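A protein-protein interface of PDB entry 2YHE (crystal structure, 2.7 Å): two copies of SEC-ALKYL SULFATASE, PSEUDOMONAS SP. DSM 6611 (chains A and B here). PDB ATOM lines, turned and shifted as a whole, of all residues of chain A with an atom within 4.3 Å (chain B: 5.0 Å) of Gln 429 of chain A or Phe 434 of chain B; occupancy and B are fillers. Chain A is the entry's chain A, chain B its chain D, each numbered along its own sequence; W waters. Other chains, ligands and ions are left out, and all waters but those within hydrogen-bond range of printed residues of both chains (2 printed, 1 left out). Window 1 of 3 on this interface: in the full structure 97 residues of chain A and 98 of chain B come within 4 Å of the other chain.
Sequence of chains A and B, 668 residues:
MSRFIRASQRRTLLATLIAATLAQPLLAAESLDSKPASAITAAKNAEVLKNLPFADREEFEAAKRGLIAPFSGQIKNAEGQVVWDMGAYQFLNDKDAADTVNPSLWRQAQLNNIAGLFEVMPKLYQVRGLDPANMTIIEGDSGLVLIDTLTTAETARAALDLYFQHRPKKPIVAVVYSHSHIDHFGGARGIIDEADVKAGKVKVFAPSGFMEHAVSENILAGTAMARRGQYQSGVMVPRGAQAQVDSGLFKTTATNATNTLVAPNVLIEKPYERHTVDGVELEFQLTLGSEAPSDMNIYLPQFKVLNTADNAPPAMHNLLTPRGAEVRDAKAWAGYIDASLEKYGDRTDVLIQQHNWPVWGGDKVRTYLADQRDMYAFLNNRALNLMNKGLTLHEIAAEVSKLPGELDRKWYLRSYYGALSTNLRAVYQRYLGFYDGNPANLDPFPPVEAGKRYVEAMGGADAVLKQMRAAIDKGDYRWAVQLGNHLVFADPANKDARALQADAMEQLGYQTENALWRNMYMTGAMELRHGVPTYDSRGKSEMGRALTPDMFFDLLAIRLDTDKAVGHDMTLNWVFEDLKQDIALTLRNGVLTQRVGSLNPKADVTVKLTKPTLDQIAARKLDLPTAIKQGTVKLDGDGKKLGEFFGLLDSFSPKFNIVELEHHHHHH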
ATOM      1  N   LEU A 320       0.397  20.496  20.691  1.00  0.00           N
ATOM      2  CA  LEU A 320       1.259  21.630  20.427  1.00  0.00           C
ATOM      3  C   LEU A 320       2.309  21.155  19.429  1.00  0.00           C
ATOM      4  O   LEU A 320       3.115  20.274  19.738  1.00  0.00           O
ATOM      5  CB  LEU A 320       1.906  22.161  21.736  1.00  0.00           C
ATOM      6  CG  LEU A 320       2.707  23.443  21.625  1.00  0.00           C
ATOM      7  CD1 LEU A 320       1.806  24.657  21.384  1.00  0.00           C
ATOM      8  CD2 LEU A 320       3.574  23.626  22.839  1.00  0.00           C
ATOM      9  N   VAL A 327      -2.240  26.443  20.591  1.00  0.00           N
ATOM     10  CA  VAL A 327      -2.527  25.190  21.316  1.00  0.00           C
ATOM     11  C   VAL A 327      -3.836  24.595  20.837  1.00  0.00           C
ATOM     12  O   VAL A 327      -4.760  25.306  20.432  1.00  0.00           O
ATOM     13  CB  VAL A 327      -2.548  25.184  22.864  1.00  0.00           C
ATOM     14  CG1 VAL A 327      -1.377  24.423  23.469  1.00  0.00           C
ATOM     15  CG2 VAL A 327      -2.762  26.542  23.470  1.00  0.00           C
ATOM     16  N   LEU A 393       3.936  22.094  34.862  1.00  0.00           N
ATOM     17  CA  LEU A 393       4.119  21.464  33.544  1.00  0.00           C
ATOM     18  C   LEU A 393       5.134  20.336  33.436  1.00  0.00           C
ATOM     19  O   LEU A 393       4.811  19.273  32.880  1.00  0.00           O
ATOM     20  CB  LEU A 393       4.252  22.493  32.408  1.00  0.00           C
ATOM     21  CG  LEU A 393       5.568  23.274  32.256  1.00  0.00           C
ATOM     22  CD1 LEU A 393       5.643  23.924  30.870  1.00  0.00           C
ATOM     23  CD2 LEU A 393       5.728  24.353  33.347  1.00  0.00           C
ATOM     24  N   ARG A 425       2.285  18.870  28.790  1.00  0.00           N
ATOM     25  CA  ARG A 425       2.780  20.240  28.976  1.00  0.00           C
ATOM     26  C   ARG A 425       1.877  21.239  28.234  1.00  0.00           C
ATOM     27  O   ARG A 425       1.640  22.335  28.737  1.00  0.00           O
ATOM     28  CB  ARG A 425       4.266  20.368  28.558  1.00  0.00           C
ATOM     29  CG  ARG A 425       5.220  19.670  29.510  1.00  0.00           C
ATOM     30  CD  ARG A 425       6.680  19.903  29.204  1.00  0.00           C
ATOM     31  NE  ARG A 425       7.305  18.771  28.522  1.00  0.00           N
ATOM     32  CZ  ARG A 425       8.349  18.079  28.976  1.00  0.00           C
ATOM     33  NH1 ARG A 425       8.862  18.341  30.167  1.00  0.00           N
ATOM     34  NH2 ARG A 425       8.875  17.113  28.248  1.00  0.00           N
ATOM     35  N   ALA A 426       1.335  20.829  27.073  1.00  0.00           N
ATOM     36  CA  ALA A 426       0.429  21.614  26.216  1.00  0.00           C
ATOM     37  C   ALA A 426      -0.920  21.881  26.859  1.00  0.00           C
ATOM     38  O   ALA A 426      -1.476  22.962  26.659  1.00  0.00           O
ATOM     39  CB  ALA A 426       0.248  20.926  24.875  1.00  0.00           C
ATOM     40  N   VAL A 427      -1.451  20.908  27.634  1.00  0.00           N
ATOM     41  CA  VAL A 427      -2.721  21.073  28.367  1.00  0.00           C
ATOM     42  C   VAL A 427      -2.491  22.144  29.433  1.00  0.00           C
ATOM     43  O   VAL A 427      -3.286  23.088  29.507  1.00  0.00           O
ATOM     44  CB  VAL A 427      -3.304  19.748  28.944  1.00  0.00           C
ATOM     45  CG1 VAL A 427      -4.634  19.984  29.657  1.00  0.00           C
ATOM     46  CG2 VAL A 427      -3.488  18.703  27.859  1.00  0.00           C
ATOM     47  N   TYR A 428      -1.362  22.039  30.199  1.00  0.00           N
ATOM     48  CA  TYR A 428      -0.935  23.034  31.180  1.00  0.00           C
ATOM     49  C   TYR A 428      -0.855  24.409  30.507  1.00  0.00           C
ATOM     50  O   TYR A 428      -1.388  25.379  31.036  1.00  0.00           O
ATOM     51  CB  TYR A 428       0.438  22.657  31.775  1.00  0.00           C
ATOM     52  CG  TYR A 428       0.837  23.501  32.970  1.00  0.00           C
ATOM     53  CD1 TYR A 428       1.423  24.754  32.801  1.00  0.00           C
ATOM     54  CD2 TYR A 428       0.591  23.066  34.268  1.00  0.00           C
ATOM     55  CE1 TYR A 428       1.768  25.546  33.901  1.00  0.00           C
ATOM     56  CE2 TYR A 428       0.927  23.847  35.370  1.00  0.00           C
ATOM     57  CZ  TYR A 428       1.544  25.073  35.184  1.00  0.00           C
ATOM     58  OH  TYR A 428       1.888  25.830  36.282  1.00  0.00           O
ATOM     59  N   GLN A 429      -0.230  24.477  29.316  1.00  0.00           N
ATOM     60  CA  GLN A 429      -0.097  25.716  28.563  1.00  0.00           C
ATOM     61  C   GLN A 429      -1.449  26.281  28.219  1.00  0.00           C
ATOM     62  O   GLN A 429      -1.660  27.486  28.410  1.00  0.00           O
ATOM     63  CB  GLN A 429       0.723  25.512  27.293  1.00  0.00           C
ATOM     64  CG  GLN A 429       0.880  26.830  26.497  1.00  0.00           C
ATOM     65  CD  GLN A 429       1.432  26.659  25.121  1.00  0.00           C
ATOM     66  OE1 GLN A 429       2.543  26.153  24.926  1.00  0.00           O
ATOM     67  NE2 GLN A 429       0.667  27.097  24.137  1.00  0.00           N
ATOM     68  N   ARG A 430      -2.374  25.429  27.733  1.00  0.00           N
ATOM     69  CA  ARG A 430      -3.707  25.891  27.329  1.00  0.00           C
ATOM     70  C   ARG A 430      -4.465  26.542  28.467  1.00  0.00           C
ATOM     71  O   ARG A 430      -4.974  27.646  28.306  1.00  0.00           O
ATOM     72  CB  ARG A 430      -4.542  24.751  26.723  1.00  0.00           C
ATOM     73  CG  ARG A 430      -5.717  25.269  25.907  1.00  0.00           C
ATOM     74  CD  ARG A 430      -6.603  24.186  25.357  1.00  0.00           C
ATOM     75  NE  ARG A 430      -7.764  23.961  26.217  1.00  0.00           N
ATOM     76  CZ  ARG A 430      -8.932  24.581  26.079  1.00  0.00           C
ATOM     77  NH1 ARG A 430      -9.099  25.497  25.124  1.00  0.00           N
ATOM     78  NH2 ARG A 430      -9.932  24.315  26.910  1.00  0.00           N
ATOM     79  N   TYR A 431      -4.549  25.850  29.608  1.00  0.00           N
ATOM     80  CA  TYR A 431      -5.301  26.292  30.771  1.00  0.00           C
ATOM     81  C   TYR A 431      -4.606  27.365  31.588  1.00  0.00           C
ATOM     82  O   TYR A 431      -5.285  28.291  32.047  1.00  0.00           O
ATOM     83  CB  TYR A 431      -5.652  25.075  31.653  1.00  0.00           C
ATOM     84  CG  TYR A 431      -6.744  24.211  31.072  1.00  0.00           C
ATOM     85  CD1 TYR A 431      -8.086  24.539  31.248  1.00  0.00           C
ATOM     86  CD2 TYR A 431      -6.442  23.072  30.340  1.00  0.00           C
ATOM     87  CE1 TYR A 431      -9.104  23.752  30.705  1.00  0.00           C
ATOM     88  CE2 TYR A 431      -7.453  22.261  29.808  1.00  0.00           C
ATOM     89  CZ  TYR A 431      -8.787  22.614  29.977  1.00  0.00           C
ATOM     90  OH  TYR A 431      -9.798  21.820  29.466  1.00  0.00           O
ATOM     91  N   LEU A 432      -3.269  27.223  31.820  1.00  0.00           N
ATOM     92  CA  LEU A 432      -2.530  28.143  32.687  1.00  0.00           C
ATOM     93  C   LEU A 432      -1.477  29.016  32.026  1.00  0.00           C
ATOM     94  O   LEU A 432      -1.336  30.179  32.423  1.00  0.00           O
ATOM     95  CB  LEU A 432      -1.978  27.441  33.943  1.00  0.00           C
ATOM     96  CG  LEU A 432      -2.949  26.550  34.742  1.00  0.00           C
ATOM     97  CD1 LEU A 432      -2.202  25.707  35.744  1.00  0.00           C
ATOM     98  CD2 LEU A 432      -4.046  27.379  35.425  1.00  0.00           C
ATOM     99  N   GLY A 433      -0.744  28.461  31.063  1.00  0.00           N
ATOM    100  CA  GLY A 433       0.312  29.191  30.360  1.00  0.00           C
ATOM    101  C   GLY A 433       1.710  28.672  30.632  1.00  0.00           C
ATOM    102  O   GLY A 433       1.886  27.653  31.321  1.00  0.00           O
ATOM    103  N   PHE A 434       2.714  29.367  30.100  1.00  0.00           N
ATOM    104  CA  PHE A 434       4.121  28.977  30.247  1.00  0.00           C
ATOM    105  C   PHE A 434       4.653  29.190  31.694  1.00  0.00           C
ATOM    106  O   PHE A 434       5.669  28.586  32.065  1.00  0.00           O
ATOM    107  CB  PHE A 434       4.979  29.782  29.244  1.00  0.00           C
ATOM    108  CG  PHE A 434       5.270  31.201  29.697  1.00  0.00           C
ATOM    109  CD1 PHE A 434       6.398  31.488  30.468  1.00  0.00           C
ATOM    110  CD2 PHE A 434       4.410  32.244  29.370  1.00  0.00           C
ATOM    111  CE1 PHE A 434       6.645  32.786  30.912  1.00  0.00           C
ATOM    112  CE2 PHE A 434       4.680  33.544  29.785  1.00  0.00           C
ATOM    113  CZ  PHE A 434       5.785  33.806  30.564  1.00  0.00           C
ATOM    114  N   LEU B 393      11.028  33.456  23.168  1.00  0.00           N
ATOM    115  CA  LEU B 393      10.250  34.166  24.196  1.00  0.00           C
ATOM    116  C   LEU B 393      11.014  35.067  25.168  1.00  0.00           C
ATOM    117  O   LEU B 393      10.627  36.229  25.353  1.00  0.00           O
ATOM    118  CB  LEU B 393       9.232  33.255  24.910  1.00  0.00           C
ATOM    119  CG  LEU B 393       9.712  32.240  25.934  1.00  0.00           C
ATOM    120  CD1 LEU B 393       8.571  31.774  26.746  1.00  0.00           C
ATOM    121  CD2 LEU B 393      10.420  31.035  25.273  1.00  0.00           C
ATOM    122  N   GLN B 429       3.801  32.566  23.183  1.00  0.00           N
ATOM    123  CA  GLN B 429       3.042  31.415  23.632  1.00  0.00           C
ATOM    124  C   GLN B 429       1.839  31.177  22.721  1.00  0.00           C
ATOM    125  O   GLN B 429       1.606  30.030  22.306  1.00  0.00           O
ATOM    126  CB  GLN B 429       2.592  31.588  25.084  1.00  0.00           C
ATOM    127  CG  GLN B 429       1.792  30.376  25.576  1.00  0.00           C
ATOM    128  CD  GLN B 429       1.113  30.590  26.896  1.00  0.00           C
ATOM    129  OE1 GLN B 429       1.731  30.850  27.921  1.00  0.00           O
ATOM    130  NE2 GLN B 429      -0.180  30.421  26.902  1.00  0.00           N
ATOM    131  N   LEU B 432       3.328  30.281  18.943  1.00  0.00           N
ATOM    132  CA  LEU B 432       4.248  29.153  18.872  1.00  0.00           C
ATOM    133  C   LEU B 432       4.200  28.163  20.037  1.00  0.00           C
ATOM    134  O   LEU B 432       4.356  26.963  19.801  1.00  0.00           O
ATOM    135  CB  LEU B 432       5.706  29.582  18.585  1.00  0.00           C
ATOM    136  CG  LEU B 432       5.939  30.632  17.450  1.00  0.00           C
ATOM    137  CD1 LEU B 432       7.316  31.165  17.487  1.00  0.00           C
ATOM    138  CD2 LEU B 432       5.596  30.104  16.031  1.00  0.00           C
ATOM    139  N   GLY B 433       4.019  28.653  21.264  1.00  0.00           N
ATOM    140  CA  GLY B 433       3.952  27.799  22.451  1.00  0.00           C
ATOM    141  C   GLY B 433       5.103  27.987  23.424  1.00  0.00           C
ATOM    142  O   GLY B 433       5.937  28.874  23.228  1.00  0.00           O
ATOM    143  N   PHE B 434       5.148  27.168  24.493  1.00  0.00           N
ATOM    144  CA  PHE B 434       6.188  27.223  25.547  1.00  0.00           C
ATOM    145  C   PHE B 434       7.559  26.739  25.016  1.00  0.00           C
ATOM    146  O   PHE B 434       8.602  27.050  25.616  1.00  0.00           O
ATOM    147  CB  PHE B 434       5.776  26.379  26.805  1.00  0.00           C
ATOM    148  CG  PHE B 434       5.933  24.886  26.618  1.00  0.00           C
ATOM    149  CD1 PHE B 434       4.914  24.127  26.041  1.00  0.00           C
ATOM    150  CD2 PHE B 434       7.145  24.257  26.899  1.00  0.00           C
ATOM    151  CE1 PHE B 434       5.081  22.757  25.787  1.00  0.00           C
ATOM    152  CE2 PHE B 434       7.321  22.882  26.640  1.00  0.00           C
ATOM    153  CZ  PHE B 434       6.285  22.142  26.080  1.00  0.00           C
ATOM    154  N   TYR B 435       7.529  25.895  23.967  1.00  0.00           N
ATOM    155  CA  TYR B 435       8.738  25.303  23.410  1.00  0.00           C
ATOM    156  C   TYR B 435       9.384  26.231  22.410  1.00  0.00           C
ATOM    157  O   TYR B 435       8.733  26.648  21.448  1.00  0.00           O
ATOM    158  CB  TYR B 435       8.475  23.890  22.876  1.00  0.00           C
ATOM    159  CG  TYR B 435       9.639  23.276  22.147  1.00  0.00           C
ATOM    160  CD1 TYR B 435      10.854  23.056  22.794  1.00  0.00           C
ATOM    161  CD2 TYR B 435       9.530  22.910  20.806  1.00  0.00           C
ATOM    162  CE1 TYR B 435      11.938  22.504  22.114  1.00  0.00           C
ATOM    163  CE2 TYR B 435      10.607  22.353  20.122  1.00  0.00           C
ATOM    164  CZ  TYR B 435      11.800  22.139  20.781  1.00  0.00           C
ATOM    165  OH  TYR B 435      12.840  21.571  20.092  1.00  0.00           O
ATOM    166  N   ASP B 436      10.658  26.587  22.665  1.00  0.00           N
ATOM    167  CA  ASP B 436      11.381  27.551  21.855  1.00  0.00           C
ATOM    168  C   ASP B 436      11.994  27.072  20.535  1.00  0.00           C
ATOM    169  O   ASP B 436      12.605  27.864  19.815  1.00  0.00           O
ATOM    170  CB  ASP B 436      12.397  28.310  22.716  1.00  0.00           C
ATOM    171  CG  ASP B 436      13.621  27.515  23.092  1.00  0.00           C
ATOM    172  OD1 ASP B 436      13.608  26.265  22.896  1.00  0.00           O
ATOM    173  OD2 ASP B 436      14.592  28.133  23.579  1.00  0.00           O
HETATM  174  O   HOH W   1      -1.665  29.087  24.483  1.00  0.00           O
HETATM  175  O   HOH W   2      -2.735  30.124  28.672  1.00  0.00           O
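The backbone NH (N) of Phe 434 of chain B is in hydrogen-bond range of the side-chain amide oxygen (OE1) of Gln 429 of chain A, 2.8 Å away. OE1 of Gln 429 of chain B lies within hydrogen-bond range of N of Phe 434 of chain A.
The backbone carbonyl oxygen (O) of Tyr 428 of chain A lies within hydrogen-bond range of the backbone NH (N) of Gly 433 of chain A, 3.1 Å away.
Among the printed residues, pairs that only touch across the chains: Leu 320 of chain A with Leu 432 of chain B (3.8 Å), Leu 320 of chain A with Gly 433 of chain B (3.95 Å), Leu 320 of chain A with Phe 434 of chain B (3.4 Å), Arg 425 of chain A with Phe 434 of chain B (3.7 Å), Gln 429 of chain A with Gln 429 of chain B (3.6 Å), Gln 429 of chain A with Gly 433 of chain B (3.3 Å) and Gly 433 of chain A with Gln 429 of chain B (3.3 Å).
Of the printed residues of chain B, Leu 320 of chain A touches Leu 432, Gly 433 and Phe 434. Gln 429 of chain A touches three residues of chain B. Leu 432 of chain A touches none of the printed residues of chain B. Printed residues of chain B within 4 Å of Gly 433 of chain A: Gln 429. Of the printed residues of chain B, Phe 434 of chain A touches Gln 429. Printed residues of chain A within 4 Å of Leu 432 of chain B: Leu 320 (3.8 Å). Printed residues of chain A within 4 Å of Gly 433 of chain B: Leu 320 and Gln 429. Of chain A, only Leu 320 (3.4 Å), Arg 425 (3.7 Å) and Gln 429 (2.8 Å) come within 4 Å of Phe 434 of chain B. The nearest printed residue of chain B that does not touch Gln 429 of chain A is Tyr 435 of chain B (5.1 Å). The nearest printed residue of chain B that does not touch Leu 320 of chain A is Tyr 435 of chain B (4.7 Å).
Of the 7 printed residues of chain B, 4 touch a printed residue of chain A. Printed residues of chain B that touch a printed residue of chain A: Gln 429, Leu 432, Gly 433 and Phe 434. Hydrophobic or aromatic side chains of chain B within 4 Å of the printed part of chain A: Phe 434. Of the 13 printed residues of chain A, 5 touch a printed residue of chain B. Along chain A the printed residues that touch a printed residue of chain B span positions 320 to 434. Among the printed residues, 9 pairs touch across the chains. Among the printed residues, no Asp or Glu carboxylate lies within 4 Å of a Lys or Arg side-chain nitrogen of the other chain.
Gln 429 of chain A touches its own counterpart, Gln 429 of chain B. Gln 429 of chain A touches Gly 433 of chain B, and with the chains exchanged Gly 433 of chain A touches Gln 429 of chain B. Gln 429 of chain A touches Phe 434 of chain B, and with the chains exchanged Phe 434 of chain A touches Gln 429 of chain B. Of the 9 pairs that touch across the chains among the printed residues, 5 have their exchanged pair printed and touching as well.
Water W2 lies within hydrogen-bond range of O of Gln 429 of chain A, NE2 of Gln 429 of chain B and O of Arg 430 of chain A. Water W1 bridges the side-chain amide nitrogen of Gln 429 of chain A (3.1 Å) and the side-chain amide nitrogen of Gln 429 of chain B (3.1 Å).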
